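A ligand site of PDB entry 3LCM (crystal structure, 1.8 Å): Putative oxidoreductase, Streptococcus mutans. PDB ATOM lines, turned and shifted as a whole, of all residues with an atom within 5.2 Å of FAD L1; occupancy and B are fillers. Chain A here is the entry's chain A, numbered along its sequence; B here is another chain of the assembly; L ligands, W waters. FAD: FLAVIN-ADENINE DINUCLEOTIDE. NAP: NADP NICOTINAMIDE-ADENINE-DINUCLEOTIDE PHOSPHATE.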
ATOM      1  N   HIS A   9      28.798  20.201   8.436  1.00  0.00           N
ATOM      2  CA  HIS A   9      28.531  19.264   9.518  1.00  0.00           C
ATOM      3  C   HIS A   9      29.814  18.934  10.277  1.00  0.00           C
ATOM      4  O   HIS A   9      30.844  18.676   9.662  1.00  0.00           O
ATOM      5  CB  HIS A   9      27.851  17.973   9.021  1.00  0.00           C
ATOM      6  CG  HIS A   9      27.181  17.198  10.115  1.00  0.00           C
ATOM      7  ND1 HIS A   9      27.880  16.474  11.053  1.00  0.00           N
ATOM      8  CD2 HIS A   9      25.866  17.076  10.442  1.00  0.00           C
ATOM      9  CE1 HIS A   9      27.039  15.926  11.907  1.00  0.00           C
ATOM     10  NE2 HIS A   9      25.811  16.267  11.560  1.00  0.00           N
ATOM     11  N   ASN A  11      30.608  16.354  12.131  1.00  0.00           N
ATOM     12  CA  ASN A  11      30.942  14.925  12.208  1.00  0.00           C
ATOM     13  C   ASN A  11      31.221  14.268  10.863  1.00  0.00           C
ATOM     14  O   ASN A  11      30.318  14.109  10.041  1.00  0.00           O
ATOM     15  CB  ASN A  11      29.833  14.150  12.925  1.00  0.00           C
ATOM     16  CG  ASN A  11      30.161  12.681  13.107  1.00  0.00           C
ATOM     17  OD1 ASN A  11      31.324  12.269  12.983  1.00  0.00           O
ATOM     18  ND2 ASN A  11      29.150  11.888  13.420  1.00  0.00           N
ATOM     19  N   THR A  13      31.649  11.301  10.183  1.00  0.00           N
ATOM     20  CA  THR A  13      30.903  10.058  10.005  1.00  0.00           C
ATOM     21  C   THR A  13      29.392  10.279  10.108  1.00  0.00           C
ATOM     22  O   THR A  13      28.634   9.373  10.448  1.00  0.00           O
ATOM     23  CB  THR A  13      31.399   8.955  10.997  1.00  0.00           C
ATOM     24  OG1 THR A  13      31.154   9.356  12.348  1.00  0.00           O
ATOM     25  CG2 THR A  13      32.877   8.706  10.813  1.00  0.00           C
ATOM     26  N   SER A  14      28.950  11.494   9.783  1.00  0.00           N
ATOM     27  CA  SER A  14      27.539  11.844   9.847  1.00  0.00           C
ATOM     28  C   SER A  14      26.792  11.379   8.596  1.00  0.00           C
ATOM     29  O   SER A  14      27.403  10.949   7.613  1.00  0.00           O
ATOM     30  CB  SER A  14      27.345  13.355  10.071  1.00  0.00           C
ATOM     31  OG  SER A  14      27.814  14.113   8.968  1.00  0.00           O
ATOM     32  N   PHE A  15      25.466  11.431   8.655  1.00  0.00           N
ATOM     33  CA  PHE A  15      24.640  11.122   7.484  1.00  0.00           C
ATOM     34  C   PHE A  15      24.859  12.203   6.423  1.00  0.00           C
ATOM     35  O   PHE A  15      24.846  11.921   5.221  1.00  0.00           O
ATOM     36  CB  PHE A  15      23.168  11.034   7.901  1.00  0.00           C
ATOM     37  CG  PHE A  15      22.251  10.649   6.796  1.00  0.00           C
ATOM     38  CD1 PHE A  15      22.254   9.341   6.293  1.00  0.00           C
ATOM     39  CD2 PHE A  15      21.352  11.567   6.262  1.00  0.00           C
ATOM     40  CE1 PHE A  15      21.401   8.974   5.273  1.00  0.00           C
ATOM     41  CE2 PHE A  15      20.490  11.202   5.245  1.00  0.00           C
ATOM     42  CZ  PHE A  15      20.519   9.900   4.751  1.00  0.00           C
ATOM     43  N   ASN A  16      25.034  13.462   6.848  1.00  0.00           N
ATOM     44  CA  ASN A  16      25.362  14.566   5.937  1.00  0.00           C
ATOM     45  C   ASN A  16      26.657  14.295   5.192  1.00  0.00           C
ATOM     46  O   ASN A  16      26.784  14.585   4.074  1.00  0.00           O
ATOM     47  CB  ASN A  16      25.405  15.919   6.644  1.00  0.00           C
ATOM     48  CG  ASN A  16      24.065  16.575   6.724  1.00  0.00           C
ATOM     49  OD1 ASN A  16      23.802  17.480   6.039  1.00  0.00           O
ATOM     50  ND2 ASN A  16      23.231  16.088   7.562  1.00  0.00           N
ATOM     51  N   ALA A  17      27.630  13.702   5.868  1.00  0.00           N
ATOM     52  CA  ALA A  17      28.894  13.343   5.245  1.00  0.00           C
ATOM     53  C   ALA A  17      28.646  12.359   4.110  1.00  0.00           C
ATOM     54  O   ALA A  17      29.266  12.439   3.056  1.00  0.00           O
ATOM     55  CB  ALA A  17      29.846  12.748   6.275  1.00  0.00           C
ATOM     56  N   GLU A  18      27.727  11.430   4.338  1.00  0.00           N
ATOM     57  CA  GLU A  18      27.376  10.437   3.320  1.00  0.00           C
ATOM     58  C   GLU A  18      26.611  11.086   2.169  1.00  0.00           C
ATOM     59  O   GLU A  18      26.748  10.678   1.013  1.00  0.00           O
ATOM     60  CB  GLU A  18      26.586   9.284   3.945  1.00  0.00           C
ATOM     61  CG  GLU A  18      26.171   8.184   2.963  1.00  0.00           C
ATOM     62  CD  GLU A  18      27.360   7.463   2.346  1.00  0.00           C
ATOM     63  OE1 GLU A  18      28.428   7.434   2.980  1.00  0.00           O
ATOM     64  OE2 GLU A  18      27.222   6.916   1.230  1.00  0.00           O
ATOM     65  N   PRO A  82      22.414  19.992   7.964  1.00  0.00           N
ATOM     66  CA  PRO A  82      21.291  19.617   8.830  1.00  0.00           C
ATOM     67  C   PRO A  82      20.573  20.855   9.332  1.00  0.00           C
ATOM     68  O   PRO A  82      21.201  21.900   9.512  1.00  0.00           O
ATOM     69  CB  PRO A  82      21.975  18.932  10.017  1.00  0.00           C
ATOM     70  CG  PRO A  82      23.333  19.578  10.091  1.00  0.00           C
ATOM     71  CD  PRO A  82      23.717  19.936   8.670  1.00  0.00           C
ATOM     72  N   ILE A  83      19.265  20.754   9.541  1.00  0.00           N
ATOM     73  CA  ILE A  83      18.506  21.826  10.155  1.00  0.00           C
ATOM     74  C   ILE A  83      18.795  21.870  11.655  1.00  0.00           C
ATOM     75  O   ILE A  83      18.584  20.884  12.360  1.00  0.00           O
ATOM     76  CB  ILE A  83      16.985  21.639   9.946  1.00  0.00           C
ATOM     77  CG1 ILE A  83      16.617  21.835   8.471  1.00  0.00           C
ATOM     78  CG2 ILE A  83      16.192  22.615  10.838  1.00  0.00           C
ATOM     79  CD1 ILE A  83      17.093  23.154   7.865  1.00  0.00           C
ATOM     80  N   TRP A  84      19.304  23.004  12.128  1.00  0.00           N
ATOM     81  CA  TRP A  84      19.469  23.231  13.560  1.00  0.00           C
ATOM     82  C   TRP A  84      18.613  24.426  13.938  1.00  0.00           C
ATOM     83  O   TRP A  84      18.844  25.531  13.441  1.00  0.00           O
ATOM     84  CB  TRP A  84      20.924  23.500  13.939  1.00  0.00           C
ATOM     85  CG  TRP A  84      21.861  22.320  13.793  1.00  0.00           C
ATOM     86  CD1 TRP A  84      21.514  21.019  13.526  1.00  0.00           C
ATOM     87  CD2 TRP A  84      23.277  22.341  13.926  1.00  0.00           C
ATOM     88  NE1 TRP A  84      22.646  20.235  13.485  1.00  0.00           N
ATOM     89  CE2 TRP A  84      23.735  21.021  13.725  1.00  0.00           C
ATOM     90  CE3 TRP A  84      24.220  23.348  14.198  1.00  0.00           C
ATOM     91  CZ2 TRP A  84      25.101  20.675  13.781  1.00  0.00           C
ATOM     92  CZ3 TRP A  84      25.573  23.008  14.244  1.00  0.00           C
ATOM     93  CH2 TRP A  84      25.995  21.684  14.037  1.00  0.00           C
ATOM     94  N   TRP A  85      17.635  24.219  14.808  1.00  0.00           N
ATOM     95  CA  TRP A  85      16.751  25.291  15.213  1.00  0.00           C
ATOM     96  C   TRP A  85      16.153  26.017  13.997  1.00  0.00           C
ATOM     97  O   TRP A  85      16.300  27.235  13.850  1.00  0.00           O
ATOM     98  CB  TRP A  85      17.462  26.255  16.167  1.00  0.00           C
ATOM     99  CG  TRP A  85      17.819  25.589  17.458  1.00  0.00           C
ATOM    100  CD1 TRP A  85      19.071  25.253  17.906  1.00  0.00           C
ATOM    101  CD2 TRP A  85      16.896  25.133  18.459  1.00  0.00           C
ATOM    102  NE1 TRP A  85      18.983  24.627  19.128  1.00  0.00           N
ATOM    103  CE2 TRP A  85      17.667  24.542  19.495  1.00  0.00           C
ATOM    104  CE3 TRP A  85      15.503  25.168  18.584  1.00  0.00           C
ATOM    105  CZ2 TRP A  85      17.078  24.002  20.645  1.00  0.00           C
ATOM    106  CZ3 TRP A  85      14.922  24.626  19.731  1.00  0.00           C
ATOM    107  CH2 TRP A  85      15.709  24.052  20.738  1.00  0.00           C
ATOM    108  N   SER A  86      15.509  25.235  13.126  1.00  0.00           N
ATOM    109  CA  SER A  86      14.754  25.731  11.976  1.00  0.00           C
ATOM    110  C   SER A  86      15.576  26.303  10.823  1.00  0.00           C
ATOM    111  O   SER A  86      14.999  26.825   9.865  1.00  0.00           O
ATOM    112  CB  SER A  86      13.735  26.774  12.411  1.00  0.00           C
ATOM    113  OG  SER A  86      12.869  26.252  13.401  1.00  0.00           O
ATOM    114  N   GLY A  87      16.902  26.241  10.899  1.00  0.00           N
ATOM    115  CA  GLY A  87      17.733  26.836   9.855  1.00  0.00           C
ATOM    116  C   GLY A  87      19.169  26.386   9.803  1.00  0.00           C
ATOM    117  O   GLY A  87      19.524  25.276  10.218  1.00  0.00           O
ATOM    118  N   THR A 127      18.589  18.187   5.903  1.00  0.00           N
ATOM    119  CA  THR A 127      18.064  17.044   6.639  1.00  0.00           C
ATOM    120  C   THR A 127      17.437  17.536   7.947  1.00  0.00           C
ATOM    121  O   THR A 127      17.957  18.448   8.592  1.00  0.00           O
ATOM    122  CB  THR A 127      19.176  16.019   6.948  1.00  0.00           C
ATOM    123  OG1 THR A 127      20.242  16.662   7.657  1.00  0.00           O
ATOM    124  CG2 THR A 127      19.726  15.432   5.659  1.00  0.00           C
ATOM    125  N   HIS A 128      16.308  16.950   8.325  1.00  0.00           N
ATOM    126  CA  HIS A 128      15.741  17.243   9.654  1.00  0.00           C
ATOM    127  C   HIS A 128      14.814  16.135  10.162  1.00  0.00           C
ATOM    128  O   HIS A 128      14.597  15.139   9.478  1.00  0.00           O
ATOM    129  CB  HIS A 128      15.041  18.602   9.652  1.00  0.00           C
ATOM    130  CG  HIS A 128      13.948  18.711   8.637  1.00  0.00           C
ATOM    131  ND1 HIS A 128      12.684  18.209   8.848  1.00  0.00           N
ATOM    132  CD2 HIS A 128      13.941  19.268   7.401  1.00  0.00           C
ATOM    133  CE1 HIS A 128      11.934  18.449   7.780  1.00  0.00           C
ATOM    134  NE2 HIS A 128      12.676  19.091   6.888  1.00  0.00           N
ATOM    135  N   ASN A 129      14.302  16.342  11.354  1.00  0.00           N
ATOM    136  CA  ASN A 129      13.447  15.362  12.028  1.00  0.00           C
ATOM    137  C   ASN A 129      11.951  15.682  11.985  1.00  0.00           C
ATOM    138  O   ASN A 129      11.174  15.022  12.625  1.00  0.00           O
ATOM    139  CB  ASN A 129      13.890  15.150  13.477  1.00  0.00           C
ATOM    140  CG  ASN A 129      15.103  14.273  13.608  1.00  0.00           C
ATOM    141  OD1 ASN A 129      15.277  13.377  12.842  1.00  0.00           O
ATOM    142  ND2 ASN A 129      15.914  14.509  14.590  1.00  0.00           N
ATOM    143  N   THR A 130      11.586  16.681  11.225  1.00  0.00           N
ATOM    144  CA  THR A 130      10.207  17.175  11.197  1.00  0.00           C
ATOM    145  C   THR A 130       9.461  16.562  10.013  1.00  0.00           C
ATOM    146  O   THR A 130      10.035  16.406   8.939  1.00  0.00           O
ATOM    147  CB  THR A 130      10.181  18.716  11.132  1.00  0.00           C
ATOM    148  OG1 THR A 130      10.865  19.248  12.281  1.00  0.00           O
ATOM    149  CG2 THR A 130       8.763  19.272  11.108  1.00  0.00           C
ATOM    150  N   TYR A 141      13.358  26.547   7.725  1.00  0.00           N
ATOM    151  CA  TYR A 141      13.704  25.184   7.285  1.00  0.00           C
ATOM    152  C   TYR A 141      14.275  25.162   5.861  1.00  0.00           C
ATOM    153  O   TYR A 141      13.904  24.317   5.041  1.00  0.00           O
ATOM    154  CB  TYR A 141      12.494  24.256   7.383  1.00  0.00           C
ATOM    155  CG  TYR A 141      12.277  23.653   8.753  1.00  0.00           C
ATOM    156  CD1 TYR A 141      12.538  22.306   8.978  1.00  0.00           C
ATOM    157  CD2 TYR A 141      11.817  24.423   9.808  1.00  0.00           C
ATOM    158  CE1 TYR A 141      12.355  21.746  10.229  1.00  0.00           C
ATOM    159  CE2 TYR A 141      11.625  23.865  11.062  1.00  0.00           C
ATOM    160  CZ  TYR A 141      11.901  22.526  11.263  1.00  0.00           C
ATOM    161  OH  TYR A 141      11.701  21.966  12.495  1.00  0.00           O
ATOM    162  N   ILE A 166      14.239  12.398   9.230  1.00  0.00           N
ATOM    163  CA  ILE A 166      15.487  11.751   8.807  1.00  0.00           C
ATOM    164  C   ILE A 166      16.021  10.757   9.840  1.00  0.00           C
ATOM    165  O   ILE A 166      16.733   9.805   9.491  1.00  0.00           O
ATOM    166  CB  ILE A 166      16.568  12.804   8.438  1.00  0.00           C
ATOM    167  CG1 ILE A 166      17.679  12.161   7.607  1.00  0.00           C
ATOM    168  CG2 ILE A 166      17.131  13.487   9.677  1.00  0.00           C
ATOM    169  CD1 ILE A 166      17.183  11.524   6.346  1.00  0.00           C
ATOM    170  N   GLU A 167      15.664  10.974  11.104  1.00  0.00           N
ATOM    171  CA  GLU A 167      16.112  10.098  12.193  1.00  0.00           C
ATOM    172  C   GLU A 167      15.074   9.030  12.538  1.00  0.00           C
ATOM    173  O   GLU A 167      15.438   7.926  12.944  1.00  0.00           O
ATOM    174  CB  GLU A 167      16.490  10.930  13.425  1.00  0.00           C
ATOM    175  N   ASP A 171      16.923   2.554   8.459  1.00  0.00           N
ATOM    176  CA  ASP A 171      18.187   2.645   7.743  1.00  0.00           C
ATOM    177  C   ASP A 171      17.979   2.367   6.248  1.00  0.00           C
ATOM    178  O   ASP A 171      18.732   2.869   5.414  1.00  0.00           O
ATOM    179  CB  ASP A 171      19.226   1.683   8.340  1.00  0.00           C
ATOM    180  N   ARG A 174      16.505   5.582   4.686  1.00  0.00           N
ATOM    181  CA  ARG A 174      17.591   6.545   4.549  1.00  0.00           C
ATOM    182  C   ARG A 174      18.460   6.237   3.329  1.00  0.00           C
ATOM    183  O   ARG A 174      18.828   7.155   2.593  1.00  0.00           O
ATOM    184  CB  ARG A 174      18.457   6.593   5.814  1.00  0.00           C
ATOM    185  CG  ARG A 174      17.918   7.525   6.881  1.00  0.00           C
ATOM    186  CD  ARG A 174      18.911   7.642   8.030  1.00  0.00           C
ATOM    187  NE  ARG A 174      19.027   6.391   8.785  1.00  0.00           N
ATOM    188  CZ  ARG A 174      18.169   5.998   9.716  1.00  0.00           C
ATOM    189  NH1 ARG A 174      17.113   6.754  10.031  1.00  0.00           N
ATOM    190  NH2 ARG A 174      18.348   4.844  10.342  1.00  0.00           N
ATOM    191  N   GLN A 175      18.785   4.961   3.124  1.00  0.00           N
ATOM    192  CA  GLN A 175      19.535   4.546   1.939  1.00  0.00           C
ATOM    193  C   GLN A 175      18.756   4.887   0.656  1.00  0.00           C
ATOM    194  O   GLN A 175      19.340   5.301  -0.337  1.00  0.00           O
ATOM    195  CB  GLN A 175      19.879   3.053   1.989  1.00  0.00           C
ATOM    196  N   LEU A 178      19.440   8.418  -0.038  1.00  0.00           N
ATOM    197  CA  LEU A 178      20.745   8.580  -0.677  1.00  0.00           C
ATOM    198  C   LEU A 178      20.641   8.297  -2.180  1.00  0.00           C
ATOM    199  O   LEU A 178      21.281   8.990  -2.992  1.00  0.00           O
ATOM    200  CB  LEU A 178      21.795   7.669  -0.017  1.00  0.00           C
ATOM    201  CG  LEU A 178      22.044   7.960   1.463  1.00  0.00           C
ATOM    202  CD1 LEU A 178      23.038   6.979   2.067  1.00  0.00           C
ATOM    203  CD2 LEU A 178      22.507   9.377   1.652  1.00  0.00           C
ATOM    204  N   LEU B  47      29.148  24.807  16.972  1.00  0.00           N
ATOM    205  CA  LEU B  47      28.809  23.565  17.682  1.00  0.00           C
ATOM    206  C   LEU B  47      29.650  22.397  17.180  1.00  0.00           C
ATOM    207  O   LEU B  47      29.682  22.125  15.976  1.00  0.00           O
ATOM    208  CB  LEU B  47      27.322  23.239  17.533  1.00  0.00           C
ATOM    209  CG  LEU B  47      26.797  21.971  18.219  1.00  0.00           C
ATOM    210  CD1 LEU B  47      27.027  22.022  19.731  1.00  0.00           C
ATOM    211  CD2 LEU B  47      25.330  21.752  17.903  1.00  0.00           C
ATOM    212  N   PHE B  49      30.565  18.257  17.604  1.00  0.00           N
ATOM    213  CA  PHE B  49      30.269  16.982  18.111  1.00  0.00           C
ATOM    214  C   PHE B  49      30.658  15.918  17.096  1.00  0.00           C
ATOM    215  O   PHE B  49      30.838  16.215  15.972  1.00  0.00           O
ATOM    216  CB  PHE B  49      28.820  16.855  18.619  1.00  0.00           C
ATOM    217  CG  PHE B  49      27.774  16.960  17.559  1.00  0.00           C
ATOM    218  CD1 PHE B  49      27.459  15.871  16.802  1.00  0.00           C
ATOM    219  CD2 PHE B  49      27.147  18.126  17.288  1.00  0.00           C
ATOM    220  CE1 PHE B  49      26.493  15.950  15.834  1.00  0.00           C
ATOM    221  CE2 PHE B  49      26.200  18.210  16.309  1.00  0.00           C
ATOM    222  CZ  PHE B  49      25.877  17.106  15.603  1.00  0.00           C
ATOM    223  N   ARG B  55      27.072  13.973  20.792  1.00  0.00           N
ATOM    224  CA  ARG B  55      26.063  14.950  20.820  1.00  0.00           C
ATOM    225  C   ARG B  55      25.262  14.824  22.102  1.00  0.00           C
ATOM    226  O   ARG B  55      24.768  15.768  22.530  1.00  0.00           O
ATOM    227  CB  ARG B  55      25.161  14.830  19.591  1.00  0.00           C
ATOM    228  CG  ARG B  55      23.828  15.465  19.770  1.00  0.00           C
ATOM    229  CD  ARG B  55      23.244  16.214  18.648  1.00  0.00           C
ATOM    230  NE  ARG B  55      22.511  15.315  17.777  1.00  0.00           N
ATOM    231  CZ  ARG B  55      21.202  15.307  17.572  1.00  0.00           C
ATOM    232  NH1 ARG B  55      20.690  14.413  16.748  1.00  0.00           N
ATOM    233  NH2 ARG B  55      20.411  16.133  18.151  1.00  0.00           N
ATOM    234  N   ASP B  97      22.488  27.164  19.419  1.00  0.00           N
ATOM    235  CA  ASP B  97      22.999  25.851  19.023  1.00  0.00           C
ATOM    236  C   ASP B  97      23.726  25.168  20.176  1.00  0.00           C
ATOM    237  O   ASP B  97      23.505  23.998  20.455  1.00  0.00           O
ATOM    238  CB  ASP B  97      23.960  25.957  17.843  1.00  0.00           C
ATOM    239  CG  ASP B  97      23.276  26.329  16.534  1.00  0.00           C
ATOM    240  OD1 ASP B  97      22.024  26.325  16.466  1.00  0.00           O
ATOM    241  OD2 ASP B  97      24.015  26.629  15.566  1.00  0.00           O
HETATM  242  PA  FAD L   1      23.477  11.505  12.036  1.00  0.00           P
HETATM  243  O1A FAD L   1      23.003  11.683  13.520  1.00  0.00           O
HETATM  244  O2A FAD L   1      24.846  11.523  11.901  1.00  0.00           O
HETATM  245  O5B FAD L   1      22.856  10.226  11.389  1.00  0.00           O
HETATM  246  C5B FAD L   1      21.517  10.136  11.466  1.00  0.00           C
HETATM  247  C4B FAD L   1      20.981   8.762  11.195  1.00  0.00           C
HETATM  248  O4B FAD L   1      21.304   8.232   9.901  1.00  0.00           O
HETATM  249  C3B FAD L   1      21.487   7.641  12.194  1.00  0.00           C
HETATM  250  O3B FAD L   1      20.612   6.735  12.665  1.00  0.00           O
HETATM  251  C2B FAD L   1      22.631   7.059  11.422  1.00  0.00           C
HETATM  252  O2B FAD L   1      23.240   5.907  11.884  1.00  0.00           O
HETATM  253  C1B FAD L   1      22.108   7.147  10.037  1.00  0.00           C
HETATM  254  N9A FAD L   1      23.044   6.894   8.980  1.00  0.00           N
HETATM  255  C8A FAD L   1      24.294   7.230   8.994  1.00  0.00           C
HETATM  256  N7A FAD L   1      24.897   6.809   7.856  1.00  0.00           N
HETATM  257  C5A FAD L   1      23.962   6.107   7.186  1.00  0.00           C
HETATM  258  C6A FAD L   1      24.008   5.528   5.964  1.00  0.00           C
HETATM  259  N6A FAD L   1      25.274   5.463   5.320  1.00  0.00           N
HETATM  260  N1A FAD L   1      22.981   4.870   5.476  1.00  0.00           N
HETATM  261  C2A FAD L   1      21.851   4.827   6.174  1.00  0.00           C
HETATM  262  N3A FAD L   1      21.799   5.447   7.386  1.00  0.00           N
HETATM  263  C4A FAD L   1      22.835   6.163   7.834  1.00  0.00           C
HETATM  264  N1  FAD L   1      15.528  18.725  13.704  1.00  0.00           N
HETATM  265  C2  FAD L   1      14.159  19.283  13.440  1.00  0.00           C
HETATM  266  O2  FAD L   1      13.437  18.613  12.522  1.00  0.00           O
HETATM  267  N3  FAD L   1      14.120  20.816  13.437  1.00  0.00           N
HETATM  268  C4  FAD L   1      14.898  21.571  14.567  1.00  0.00           C
HETATM  269  O4  FAD L   1      15.012  22.872  14.270  1.00  0.00           O
HETATM  270  C4X FAD L   1      16.221  20.896  14.927  1.00  0.00           C
HETATM  271  N5  FAD L   1      17.314  21.615  15.511  1.00  0.00           N
HETATM  272  C5X FAD L   1      18.485  20.925  15.940  1.00  0.00           C
HETATM  273  C6  FAD L   1      19.493  21.648  16.587  1.00  0.00           C
HETATM  274  C7  FAD L   1      20.646  21.026  16.955  1.00  0.00           C
HETATM  275  C7M FAD L   1      21.775  21.755  17.669  1.00  0.00           C
HETATM  276  C8  FAD L   1      20.835  19.771  16.649  1.00  0.00           C
HETATM  277  C8M FAD L   1      22.131  19.087  16.938  1.00  0.00           C
HETATM  278  C9  FAD L   1      19.908  19.092  15.961  1.00  0.00           C
HETATM  279  C9A FAD L   1      18.716  19.706  15.579  1.00  0.00           C
HETATM  280  N10 FAD L   1      17.823  18.957  14.778  1.00  0.00           N
HETATM  281  C10 FAD L   1      16.588  19.528  14.328  1.00  0.00           C
HETATM  282  C1' FAD L   1      18.188  17.610  14.384  1.00  0.00           C
HETATM  283  C2' FAD L   1      18.859  17.451  13.024  1.00  0.00           C
HETATM  284  O2' FAD L   1      18.379  18.281  12.030  1.00  0.00           O
HETATM  285  C3' FAD L   1      19.233  16.014  12.618  1.00  0.00           C
HETATM  286  O3' FAD L   1      19.941  15.388  13.617  1.00  0.00           O
HETATM  287  C4' FAD L   1      19.995  15.963  11.299  1.00  0.00           C
HETATM  288  O4' FAD L   1      19.303  16.509  10.304  1.00  0.00           O
HETATM  289  C5' FAD L   1      20.623  14.614  10.922  1.00  0.00           C
HETATM  290  O5' FAD L   1      21.724  14.623  10.093  1.00  0.00           O
HETATM  291  P   FAD L   1      23.123  14.126  10.661  1.00  0.00           P
HETATM  292  O1P FAD L   1      24.272  14.355   9.582  1.00  0.00           O
HETATM  293  O2P FAD L   1      23.380  14.991  11.738  1.00  0.00           O
HETATM  294  O3P FAD L   1      22.763  12.651  11.170  1.00  0.00           O
HETATM  295  N1N NAP L   2      13.808  20.752  17.094  1.00  0.00           N
HETATM  296  C2N NAP L   2      14.154  19.420  17.080  1.00  0.00           C
HETATM  297  C3N NAP L   2      15.365  19.009  17.708  1.00  0.00           C
HETATM  298  C7N NAP L   2      15.836  17.559  17.696  1.00  0.00           C
HETATM  299  O7N NAP L   2      15.168  16.689  17.286  1.00  0.00           O
HETATM  300  N7N NAP L   2      17.152  17.320  18.205  1.00  0.00           N
HETATM  301  C4N NAP L   2      16.137  19.966  18.371  1.00  0.00           C
HETATM  302  C5N NAP L   2      15.691  21.298  18.534  1.00  0.00           C
HETATM  303  C6N NAP L   2      14.566  21.739  17.821  1.00  0.00           C
HETATM  304  O   HOH W   1      13.445  25.044  15.653  1.00  0.00           O
HETATM  305  O   HOH W   2      26.499  12.886  13.419  1.00  0.00           O
HETATM  306  O   HOH W   3      23.067  14.436  14.839  1.00  0.00           O
HETATM  307  O   HOH W   4      21.093  22.984  20.524  1.00  0.00           O
HETATM  308  O   HOH W   5      22.829  16.968  13.643  1.00  0.00           O
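Merely in contact with FAD L1: Ser 14 (3.3 Å), Glu 18 (3.7 Å), Pro 82 (3.6 Å), Trp 84 (3.3 Å), His 128 (3.3 Å), Ile 166 (3.8 Å), Asp 171 (3.8 Å), Leu 47 of chain B (3.6 Å) and Asp 97 of chain B (3.97 Å).
Hydrophobic or aromatic side chains that line FAD L1: His 9, Phe 15, Pro 82, Ile 83, Trp 84, Trp 85, His 128, Tyr 141, Ile 166 and Leu 47 of chain B.
Within 4 Å of FAD L1: His 9, Ser 14, Phe 15, Asn 16, Glu 18, Pro 82, Ile 83, Trp 84, Trp 85, Ser 86, Thr 127, His 128, Asn 129, Thr 130, Tyr 141, Ile 166, Asp 171, Arg 174, Leu 47 of chain B, Arg 55 of chain B and Asp 97 of chain B.
ND1 of His 9 lies within hydrogen-bond range of OG of Ser 14, at 3.2 Å.
The backbone carbonyl oxygen (O) of His 128 is in hydrogen-bond range of the backbone NH (N) of Ile 166 (2.8 Å).
The side-chain hydroxyl (OH) of Tyr 141 is in hydrogen-bond range of the side-chain hydroxyl (OG1) of Thr 130 (2.9 Å).
The side-chain hydroxyl of Thr 127 sits at hydrogen-bond distance from the side-chain amide nitrogen of Asn 16, 3.0 Å away.
The side-chain hydroxyl (OG) of Ser 14 lies within hydrogen-bond range of the backbone NH (N) of Ala 17 (3.1 Å).
The backbone NH of Asn 11 sits at hydrogen-bond distance from a ring nitrogen (ND1) of His 9 (2.9 Å).
The side-chain amide oxygen of Asn 129 lies close to the backbone NH of Glu 167, at 3.0 Å.
The side-chain hydroxyl of Ser 14 is in hydrogen-bond range of the backbone carbonyl oxygen of Asn 11.
Water W2 bridges an oxygen (O2A) of FAD L1 and the side-chain amide nitrogen (ND2) of Asn 11.
Water W5 bridges an oxygen (O2P) of FAD L1 (2.8 Å) and the indole nitrogen (NE1) of Trp 84 (3.3 Å).
Water W1 lies within hydrogen-bond range of OG of Ser 86 (2.6 Å) and O4 of FAD L1 (3.0 Å).
Water W3 lies within hydrogen-bond range of NH1 of Arg 55 of chain B (3.0 Å) and O1A of FAD L1 (3.1 Å).
Water W4 lies within hydrogen-bond range of the backbone carbonyl oxygen of Asp 97 of chain B and the indole nitrogen of Trp 85.
The side-chain hydroxyl (OG1) of Thr 127 lies within hydrogen-bond range of an oxygen (O4') of FAD L1, at 2.8 Å.
N of Asn 16 sits at hydrogen-bond distance from O1P of FAD L1, 3.0 Å away.
The side-chain hydroxyl (OH) of Tyr 141 lies within hydrogen-bond range of a nitrogen (N3) of FAD L1 (2.8 Å).
N of Trp 85 lies within hydrogen-bond range of N5 of FAD L1 (2.7 Å).
O of Ile 83 sits at hydrogen-bond distance from O2' of FAD L1 (2.6 Å).
An oxygen (O1P) of FAD L1 is in hydrogen-bond range of the backbone NH (N) of Phe 15, at 3.3 Å.
An oxygen (O2) of FAD L1 lies within hydrogen-bond range of the backbone NH (N) of Thr 130 (3.0 Å).
The backbone carbonyl oxygen (O) of Thr 127 is in hydrogen-bond range of an oxygen (O4') of FAD L1, 2.9 Å away.
The backbone NH of Asn 129 is in hydrogen-bond range of an oxygen (O2) of FAD L1.
An oxygen (O1P) of FAD L1 lies within hydrogen-bond range of the side-chain amide nitrogen (ND2) of Asn 16.
The backbone NH of Ser 86 sits at hydrogen-bond distance from an oxygen (O4) of FAD L1.
An oxygen (O2) of FAD L1 lies within hydrogen-bond range of the side-chain hydroxyl of Thr 130, 2.7 Å away.
NH1 of Arg 55 of chain B sits at hydrogen-bond distance from O3' of FAD L1 (3.4 Å).
NE of Arg 174 sits close to O4B of FAD L1 (3.1 Å).
An oxygen (O2P) of FAD L1 is in hydrogen-bond range of a ring nitrogen (NE2) of His 9 (2.8 Å).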
